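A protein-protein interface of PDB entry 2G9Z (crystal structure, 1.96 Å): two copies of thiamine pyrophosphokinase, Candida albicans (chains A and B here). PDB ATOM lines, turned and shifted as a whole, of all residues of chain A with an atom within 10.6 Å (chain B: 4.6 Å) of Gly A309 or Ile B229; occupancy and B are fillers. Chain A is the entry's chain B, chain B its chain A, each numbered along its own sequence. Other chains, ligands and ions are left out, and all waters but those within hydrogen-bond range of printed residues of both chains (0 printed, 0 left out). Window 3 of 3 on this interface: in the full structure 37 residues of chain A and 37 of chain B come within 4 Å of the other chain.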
ATOM      1  N   GLU A  22     -35.651 -20.013 -25.339  1.00  0.00           N
ATOM      2  CA  GLU A  22     -35.341 -20.496 -24.003  1.00  0.00           C
ATOM      3  C   GLU A  22     -35.356 -19.235 -23.146  1.00  0.00           C
ATOM      4  O   GLU A  22     -34.478 -18.382 -23.268  1.00  0.00           O
ATOM      5  CB  GLU A  22     -33.957 -21.154 -23.987  1.00  0.00           C
ATOM      6  CG  GLU A  22     -33.864 -22.375 -24.893  1.00  0.00           C
ATOM      7  CD  GLU A  22     -32.540 -23.105 -24.773  1.00  0.00           C
ATOM      8  OE1 GLU A  22     -32.164 -23.484 -23.644  1.00  0.00           O
ATOM      9  OE2 GLU A  22     -31.879 -23.305 -25.812  1.00  0.00           O
ATOM     10  N   LEU A 280     -31.619 -27.298 -10.283  1.00  0.00           N
ATOM     11  CA  LEU A 280     -32.186 -28.357 -11.123  1.00  0.00           C
ATOM     12  C   LEU A 280     -30.967 -28.949 -11.820  1.00  0.00           C
ATOM     13  O   LEU A 280     -30.336 -28.287 -12.639  1.00  0.00           O
ATOM     14  CB  LEU A 280     -33.175 -27.770 -12.139  1.00  0.00           C
ATOM     15  CG  LEU A 280     -34.467 -27.227 -11.511  1.00  0.00           C
ATOM     16  CD1 LEU A 280     -34.184 -25.928 -10.758  1.00  0.00           C
ATOM     17  CD2 LEU A 280     -35.500 -26.988 -12.593  1.00  0.00           C
ATOM     18  N   LEU A 281     -30.653 -30.199 -11.495  1.00  0.00           N
ATOM     19  CA  LEU A 281     -29.445 -30.838 -12.007  1.00  0.00           C
ATOM     20  C   LEU A 281     -29.673 -32.020 -12.943  1.00  0.00           C
ATOM     21  O   LEU A 281     -30.109 -33.088 -12.522  1.00  0.00           O
ATOM     22  CB  LEU A 281     -28.595 -31.245 -10.796  1.00  0.00           C
ATOM     23  CG  LEU A 281     -28.758 -30.180  -9.692  1.00  0.00           C
ATOM     24  CD1 LEU A 281     -28.254 -30.692  -8.364  1.00  0.00           C
ATOM     25  CD2 LEU A 281     -28.034 -28.898 -10.095  1.00  0.00           C
ATOM     26  N   PRO A 282     -29.360 -31.835 -14.235  1.00  0.00           N
ATOM     27  CA  PRO A 282     -29.522 -32.864 -15.266  1.00  0.00           C
ATOM     28  C   PRO A 282     -28.356 -33.848 -15.223  1.00  0.00           C
ATOM     29  O   PRO A 282     -27.427 -33.769 -16.021  1.00  0.00           O
ATOM     30  CB  PRO A 282     -29.555 -32.042 -16.547  1.00  0.00           C
ATOM     31  CG  PRO A 282     -28.548 -30.979 -16.267  1.00  0.00           C
ATOM     32  CD  PRO A 282     -28.826 -30.587 -14.818  1.00  0.00           C
ATOM     33  N   THR A 287     -30.461 -36.399 -22.280  1.00  0.00           N
ATOM     34  CA  THR A 287     -30.146 -34.992 -22.498  1.00  0.00           C
ATOM     35  C   THR A 287     -30.503 -34.551 -23.917  1.00  0.00           C
ATOM     36  O   THR A 287     -30.442 -35.346 -24.857  1.00  0.00           O
ATOM     37  CB  THR A 287     -28.635 -34.747 -22.259  1.00  0.00           C
ATOM     38  OG1 THR A 287     -28.322 -33.369 -22.484  1.00  0.00           O
ATOM     39  CG2 THR A 287     -27.804 -35.609 -23.202  1.00  0.00           C
ATOM     40  N   PRO A 288     -30.911 -33.282 -24.089  1.00  0.00           N
ATOM     41  CA  PRO A 288     -31.054 -32.272 -23.036  1.00  0.00           C
ATOM     42  C   PRO A 288     -32.446 -32.384 -22.425  1.00  0.00           C
ATOM     43  O   PRO A 288     -33.308 -33.085 -22.949  1.00  0.00           O
ATOM     44  CB  PRO A 288     -30.896 -30.945 -23.785  1.00  0.00           C
ATOM     45  CG  PRO A 288     -30.323 -31.332 -25.133  1.00  0.00           C
ATOM     46  CD  PRO A 288     -30.978 -32.645 -25.410  1.00  0.00           C
ATOM     47  N   ILE A 289     -32.662 -31.680 -21.323  1.00  0.00           N
ATOM     48  CA  ILE A 289     -33.954 -31.692 -20.664  1.00  0.00           C
ATOM     49  C   ILE A 289     -34.579 -30.308 -20.795  1.00  0.00           C
ATOM     50  O   ILE A 289     -33.909 -29.298 -20.582  1.00  0.00           O
ATOM     51  CB  ILE A 289     -33.807 -32.083 -19.175  1.00  0.00           C
ATOM     52  CG1 ILE A 289     -33.354 -33.546 -19.081  1.00  0.00           C
ATOM     53  CG2 ILE A 289     -35.124 -31.877 -18.442  1.00  0.00           C
ATOM     54  CD1 ILE A 289     -33.273 -34.095 -17.683  1.00  0.00           C
ATOM     55  N   TRP A 303     -36.609 -23.976 -21.385  1.00  0.00           N
ATOM     56  CA  TRP A 303     -35.181 -23.825 -21.151  1.00  0.00           C
ATOM     57  C   TRP A 303     -34.493 -25.197 -21.175  1.00  0.00           C
ATOM     58  O   TRP A 303     -34.789 -26.064 -20.351  1.00  0.00           O
ATOM     59  CB  TRP A 303     -34.995 -23.141 -19.797  1.00  0.00           C
ATOM     60  CG  TRP A 303     -33.678 -22.497 -19.578  1.00  0.00           C
ATOM     61  CD1 TRP A 303     -33.227 -21.330 -20.128  1.00  0.00           C
ATOM     62  CD2 TRP A 303     -32.644 -22.956 -18.707  1.00  0.00           C
ATOM     63  NE1 TRP A 303     -31.975 -21.031 -19.645  1.00  0.00           N
ATOM     64  CE2 TRP A 303     -31.593 -22.014 -18.770  1.00  0.00           C
ATOM     65  CE3 TRP A 303     -32.505 -24.074 -17.872  1.00  0.00           C
ATOM     66  CZ2 TRP A 303     -30.416 -22.156 -18.031  1.00  0.00           C
ATOM     67  CZ3 TRP A 303     -31.335 -24.215 -17.136  1.00  0.00           C
ATOM     68  CH2 TRP A 303     -30.307 -23.262 -17.220  1.00  0.00           C
ATOM     69  N   LYS A 304     -33.577 -25.384 -22.125  1.00  0.00           N
ATOM     70  CA  LYS A 304     -32.862 -26.654 -22.284  1.00  0.00           C
ATOM     71  C   LYS A 304     -31.659 -26.747 -21.355  1.00  0.00           C
ATOM     72  O   LYS A 304     -30.770 -25.900 -21.401  1.00  0.00           O
ATOM     73  CB  LYS A 304     -32.395 -26.817 -23.735  1.00  0.00           C
ATOM     74  CG  LYS A 304     -33.520 -26.783 -24.760  1.00  0.00           C
ATOM     75  CD  LYS A 304     -32.979 -26.720 -26.180  1.00  0.00           C
ATOM     76  CE  LYS A 304     -34.098 -26.510 -27.190  1.00  0.00           C
ATOM     77  NZ  LYS A 304     -33.564 -26.231 -28.554  1.00  0.00           N
ATOM     78  N   THR A 305     -31.632 -27.779 -20.517  1.00  0.00           N
ATOM     79  CA  THR A 305     -30.538 -27.962 -19.575  1.00  0.00           C
ATOM     80  C   THR A 305     -29.801 -29.292 -19.759  1.00  0.00           C
ATOM     81  O   THR A 305     -30.410 -30.322 -20.057  1.00  0.00           O
ATOM     82  CB  THR A 305     -31.045 -27.877 -18.117  1.00  0.00           C
ATOM     83  OG1 THR A 305     -29.928 -27.927 -17.219  1.00  0.00           O
ATOM     84  CG2 THR A 305     -31.988 -29.029 -17.808  1.00  0.00           C
ATOM     85  N   GLU A 306     -28.487 -29.264 -19.566  1.00  0.00           N
ATOM     86  CA  GLU A 306     -27.674 -30.469 -19.694  1.00  0.00           C
ATOM     87  C   GLU A 306     -26.262 -30.185 -19.215  1.00  0.00           C
ATOM     88  O   GLU A 306     -25.836 -29.035 -19.194  1.00  0.00           O
ATOM     89  CB  GLU A 306     -27.624 -30.930 -21.156  1.00  0.00           C
ATOM     90  CG  GLU A 306     -26.768 -30.058 -22.075  1.00  0.00           C
ATOM     91  CD  GLU A 306     -26.843 -30.500 -23.536  1.00  0.00           C
ATOM     92  OE1 GLU A 306     -26.775 -31.719 -23.802  1.00  0.00           O
ATOM     93  OE2 GLU A 306     -26.963 -29.629 -24.417  1.00  0.00           O
ATOM     94  N   MET A 307     -25.545 -31.228 -18.813  1.00  0.00           N
ATOM     95  CA  MET A 307     -24.165 -31.057 -18.382  1.00  0.00           C
ATOM     96  C   MET A 307     -23.424 -30.692 -19.660  1.00  0.00           C
ATOM     97  O   MET A 307     -23.798 -31.146 -20.741  1.00  0.00           O
ATOM     98  CB  MET A 307     -23.623 -32.350 -17.772  1.00  0.00           C
ATOM     99  CG  MET A 307     -24.256 -32.703 -16.436  1.00  0.00           C
ATOM    100  SD  MET A 307     -24.106 -31.374 -15.196  1.00  0.00           S
ATOM    101  CE  MET A 307     -22.451 -31.662 -14.566  1.00  0.00           C
ATOM    102  N   LEU A 308     -22.390 -29.868 -19.528  1.00  0.00           N
ATOM    103  CA  LEU A 308     -21.622 -29.363 -20.666  1.00  0.00           C
ATOM    104  C   LEU A 308     -22.451 -28.292 -21.356  1.00  0.00           C
ATOM    105  O   LEU A 308     -22.176 -27.907 -22.489  1.00  0.00           O
ATOM    106  CB  LEU A 308     -21.269 -30.462 -21.674  1.00  0.00           C
ATOM    107  CG  LEU A 308     -19.912 -31.097 -21.392  1.00  0.00           C
ATOM    108  CD1 LEU A 308     -20.089 -32.087 -20.265  1.00  0.00           C
ATOM    109  CD2 LEU A 308     -19.351 -31.780 -22.632  1.00  0.00           C
ATOM    110  N   GLY A 309     -23.473 -27.821 -20.654  1.00  0.00           N
ATOM    111  CA  GLY A 309     -24.340 -26.785 -21.183  1.00  0.00           C
ATOM    112  C   GLY A 309     -24.802 -25.910 -20.034  1.00  0.00           C
ATOM    113  O   GLY A 309     -24.053 -25.683 -19.086  1.00  0.00           O
ATOM    114  N   GLN A 310     -26.032 -25.416 -20.105  1.00  0.00           N
ATOM    115  CA  GLN A 310     -26.548 -24.581 -19.031  1.00  0.00           C
ATOM    116  C   GLN A 310     -27.220 -25.422 -17.953  1.00  0.00           C
ATOM    117  O   GLN A 310     -27.956 -26.369 -18.242  1.00  0.00           O
ATOM    118  CB  GLN A 310     -27.521 -23.523 -19.578  1.00  0.00           C
ATOM    119  CG  GLN A 310     -28.404 -23.982 -20.724  1.00  0.00           C
ATOM    120  CD  GLN A 310     -29.240 -22.846 -21.305  1.00  0.00           C
ATOM    121  OE1 GLN A 310     -28.764 -21.720 -21.451  1.00  0.00           O
ATOM    122  NE2 GLN A 310     -30.482 -23.143 -21.646  1.00  0.00           N
ATOM    123  N   VAL A 311     -26.930 -25.074 -16.706  1.00  0.00           N
ATOM    124  CA  VAL A 311     -27.489 -25.752 -15.545  1.00  0.00           C
ATOM    125  C   VAL A 311     -27.975 -24.685 -14.578  1.00  0.00           C
ATOM    126  O   VAL A 311     -27.245 -23.753 -14.252  1.00  0.00           O
ATOM    127  CB  VAL A 311     -26.433 -26.622 -14.826  1.00  0.00           C
ATOM    128  CG1 VAL A 311     -26.993 -27.131 -13.495  1.00  0.00           C
ATOM    129  CG2 VAL A 311     -26.045 -27.803 -15.707  1.00  0.00           C
ATOM    130  N   SER A 312     -29.216 -24.809 -14.132  1.00  0.00           N
ATOM    131  CA  SER A 312     -29.756 -23.839 -13.203  1.00  0.00           C
ATOM    132  C   SER A 312     -29.286 -24.132 -11.786  1.00  0.00           C
ATOM    133  O   SER A 312     -29.713 -25.111 -11.169  1.00  0.00           O
ATOM    134  CB  SER A 312     -31.289 -23.847 -13.252  1.00  0.00           C
ATOM    135  OG  SER A 312     -31.836 -22.942 -12.304  1.00  0.00           O
ATOM    136  N   SER A 313     -28.382 -23.297 -11.286  1.00  0.00           N
ATOM    137  CA  SER A 313     -27.891 -23.435  -9.922  1.00  0.00           C
ATOM    138  C   SER A 313     -28.024 -22.058  -9.284  1.00  0.00           C
ATOM    139  O   SER A 313     -28.072 -21.049  -9.983  1.00  0.00           O
ATOM    140  CB  SER A 313     -26.441 -23.930  -9.885  1.00  0.00           C
ATOM    141  OG  SER A 313     -25.581 -23.097 -10.624  1.00  0.00           O
ATOM    142  N   ASN B 225     -19.910 -29.271 -13.904  1.00  0.00           N
ATOM    143  CA  ASN B 225     -20.322 -28.800 -15.217  1.00  0.00           C
ATOM    144  C   ASN B 225     -19.215 -27.926 -15.813  1.00  0.00           C
ATOM    145  O   ASN B 225     -18.819 -28.107 -16.964  1.00  0.00           O
ATOM    146  CB  ASN B 225     -21.633 -28.013 -15.112  1.00  0.00           C
ATOM    147  CG  ASN B 225     -22.161 -27.574 -16.465  1.00  0.00           C
ATOM    148  OD1 ASN B 225     -22.076 -28.311 -17.444  1.00  0.00           O
ATOM    149  ND2 ASN B 225     -22.726 -26.371 -16.521  1.00  0.00           N
ATOM    150  N   GLN B 226     -18.710 -26.988 -15.015  1.00  0.00           N
ATOM    151  CA  GLN B 226     -17.646 -26.100 -15.458  1.00  0.00           C
ATOM    152  C   GLN B 226     -16.357 -26.864 -15.772  1.00  0.00           C
ATOM    153  O   GLN B 226     -15.620 -26.496 -16.685  1.00  0.00           O
ATOM    154  CB  GLN B 226     -17.380 -25.028 -14.396  1.00  0.00           C
ATOM    155  CG  GLN B 226     -18.574 -24.103 -14.176  1.00  0.00           C
ATOM    156  CD  GLN B 226     -19.117 -23.547 -15.486  1.00  0.00           C
ATOM    157  OE1 GLN B 226     -18.369 -23.007 -16.298  1.00  0.00           O
ATOM    158  NE2 GLN B 226     -20.422 -23.677 -15.693  1.00  0.00           N
ATOM    159  N   LEU B 227     -16.086 -27.919 -15.010  1.00  0.00           N
ATOM    160  CA  LEU B 227     -14.897 -28.735 -15.237  1.00  0.00           C
ATOM    161  C   LEU B 227     -14.914 -29.253 -16.676  1.00  0.00           C
ATOM    162  O   LEU B 227     -13.923 -29.131 -17.401  1.00  0.00           O
ATOM    163  CB  LEU B 227     -14.871 -29.915 -14.256  1.00  0.00           C
ATOM    164  CG  LEU B 227     -13.748 -30.948 -14.428  1.00  0.00           C
ATOM    165  CD1 LEU B 227     -12.385 -30.292 -14.200  1.00  0.00           C
ATOM    166  CD2 LEU B 227     -13.966 -32.096 -13.445  1.00  0.00           C
ATOM    167  N   TYR B 228     -16.050 -29.820 -17.080  1.00  0.00           N
ATOM    168  CA  TYR B 228     -16.220 -30.360 -18.429  1.00  0.00           C
ATOM    169  C   TYR B 228     -16.169 -29.266 -19.496  1.00  0.00           C
ATOM    170  O   TYR B 228     -15.568 -29.448 -20.556  1.00  0.00           O
ATOM    171  CB  TYR B 228     -17.561 -31.088 -18.546  1.00  0.00           C
ATOM    172  CG  TYR B 228     -17.592 -32.498 -17.994  1.00  0.00           C
ATOM    173  CD1 TYR B 228     -16.995 -33.556 -18.686  1.00  0.00           C
ATOM    174  CD2 TYR B 228     -18.272 -32.786 -16.814  1.00  0.00           C
ATOM    175  CE1 TYR B 228     -17.087 -34.869 -18.215  1.00  0.00           C
ATOM    176  CE2 TYR B 228     -18.367 -34.092 -16.332  1.00  0.00           C
ATOM    177  CZ  TYR B 228     -17.777 -35.126 -17.041  1.00  0.00           C
ATOM    178  OH  TYR B 228     -17.907 -36.414 -16.590  1.00  0.00           O
ATOM    179  N   ILE B 229     -16.827 -28.145 -19.220  1.00  0.00           N
ATOM    180  CA  ILE B 229     -16.861 -27.026 -20.156  1.00  0.00           C
ATOM    181  C   ILE B 229     -15.475 -26.427 -20.341  1.00  0.00           C
ATOM    182  O   ILE B 229     -15.053 -26.157 -21.467  1.00  0.00           O
ATOM    183  CB  ILE B 229     -17.845 -25.918 -19.675  1.00  0.00           C
ATOM    184  CG1 ILE B 229     -19.291 -26.407 -19.821  1.00  0.00           C
ATOM    185  CG2 ILE B 229     -17.633 -24.633 -20.473  1.00  0.00           C
ATOM    186  CD1 ILE B 229     -20.337 -25.445 -19.255  1.00  0.00           C
ATOM    187  N   MET B 230     -14.759 -26.226 -19.240  1.00  0.00           N
ATOM    188  CA  MET B 230     -13.434 -25.641 -19.323  1.00  0.00           C
ATOM    189  C   MET B 230     -12.451 -26.485 -20.113  1.00  0.00           C
ATOM    190  O   MET B 230     -11.583 -25.941 -20.797  1.00  0.00           O
ATOM    191  CB  MET B 230     -12.878 -25.375 -17.923  1.00  0.00           C
ATOM    192  CG  MET B 230     -13.682 -24.340 -17.148  1.00  0.00           C
ATOM    193  SD  MET B 230     -12.951 -23.978 -15.557  1.00  0.00           S
ATOM    194  CE  MET B 230     -13.281 -25.500 -14.679  1.00  0.00           C
ATOM    195  N   ASN B 231     -12.575 -27.807 -20.025  1.00  0.00           N
ATOM    196  CA  ASN B 231     -11.657 -28.670 -20.755  1.00  0.00           C
ATOM    197  C   ASN B 231     -11.983 -28.634 -22.231  1.00  0.00           C
ATOM    198  O   ASN B 231     -11.101 -28.752 -23.076  1.00  0.00           O
ATOM    199  CB  ASN B 231     -11.725 -30.120 -20.273  1.00  0.00           C
ATOM    200  CG  ASN B 231     -10.660 -30.985 -20.922  1.00  0.00           C
ATOM    201  OD1 ASN B 231      -9.469 -30.737 -20.756  1.00  0.00           O
ATOM    202  ND2 ASN B 231     -11.083 -31.992 -21.678  1.00  0.00           N
ATOM    203  N   GLU B 232     -13.264 -28.484 -22.538  1.00  0.00           N
ATOM    204  CA  GLU B 232     -13.700 -28.419 -23.920  1.00  0.00           C
ATOM    205  C   GLU B 232     -13.199 -27.112 -24.543  1.00  0.00           C
ATOM    206  O   GLU B 232     -12.677 -27.101 -25.658  1.00  0.00           O
ATOM    207  CB  GLU B 232     -15.227 -28.488 -23.973  1.00  0.00           C
ATOM    208  CG  GLU B 232     -15.817 -28.499 -25.370  1.00  0.00           C
ATOM    209  CD  GLU B 232     -17.307 -28.779 -25.357  1.00  0.00           C
ATOM    210  OE1 GLU B 232     -17.695 -29.899 -24.968  1.00  0.00           O
ATOM    211  OE2 GLU B 232     -18.091 -27.881 -25.732  1.00  0.00           O
ATOM    212  N   ASP B 233     -13.333 -26.021 -23.797  1.00  0.00           N
ATOM    213  CA  ASP B 233     -12.926 -24.707 -24.271  1.00  0.00           C
ATOM    214  C   ASP B 233     -11.464 -24.323 -24.061  1.00  0.00           C
ATOM    215  O   ASP B 233     -10.886 -23.616 -24.893  1.00  0.00           O
ATOM    216  CB  ASP B 233     -13.819 -23.631 -23.644  1.00  0.00           C
ATOM    217  CG  ASP B 233     -15.251 -23.709 -24.130  1.00  0.00           C
ATOM    218  OD1 ASP B 233     -15.499 -24.397 -25.143  1.00  0.00           O
ATOM    219  OD2 ASP B 233     -16.127 -23.073 -23.508  1.00  0.00           O
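OD1 of Asn B225 touches C of Met A307, at 3.5 Å.
Tyr B228 touches Leu A308 (CB to CD1, 3.2 Å).
CA of Leu A308 touches CG1 of Ile B229, 3.9 Å away.
OE1 of Glu B232 touches CD2 of Leu A308, 3.4 Å away.
Gly A309 touches Ile B229 (O to CD1, 3.7 Å).
CG2 of Val A311 touches ND2 of Asn B225, 3.7 Å away.
Printed residues of chain B within 4 Å of Met A307: Asn B225.
Of the printed residues of chain B, Leu A308 touches Asn B225, Tyr B228, Ile B229 and Glu B232.
Of chain B, only Asn B225 (3.0 Å) and Ile B229 (3.7 Å) come within 4 Å of Gly A309.
No residue of chain A comes within 4 Å of Gln B226.
Ile B229 touches just these residues of chain A: Leu A308 (3.9 Å) and Gly A309 (3.7 Å).
No residue of chain A comes within 4 Å of Met B230.
No residue of chain A comes within 4 Å of Asp B233.
The nearest printed residue of chain B that does not touch Gly A309 is Gln B226 (5.4 Å).
The nearest residue of chain A that does not touch Ile B229 is Gln A310 (5.8 Å).
The nearest printed residue of chain B that does not touch Val A311 is Gln B226 (6.7 Å).
Of the 9 printed residues of chain B, 4 touch a printed residue of chain A.
Printed residues of chain B that touch a printed residue of chain A: Asn B225, Tyr B228, Ile B229 and Glu B232.
Hydrophobic or aromatic side chains of chain B that line the printed part of chain A: Tyr B228 and Ile B229.
Among the printed residues, no Asp or Glu carboxylate lies within 4 Å of a Lys or Arg side-chain nitrogen of the other chain.
No position is printed for both chains.
Of the 8 pairs that touch across the chains among the printed residues, none has its exchanged pair printed and touching as well.
The side-chain amide oxygen of Asn B225 lies within hydrogen-bond range of the backbone NH of Leu A308 (2.6 Å).
The backbone carbonyl oxygen (O) of Gly A309 lies within hydrogen-bond range of the side-chain amide nitrogen (ND2) of Asn B225 (3.0 Å).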
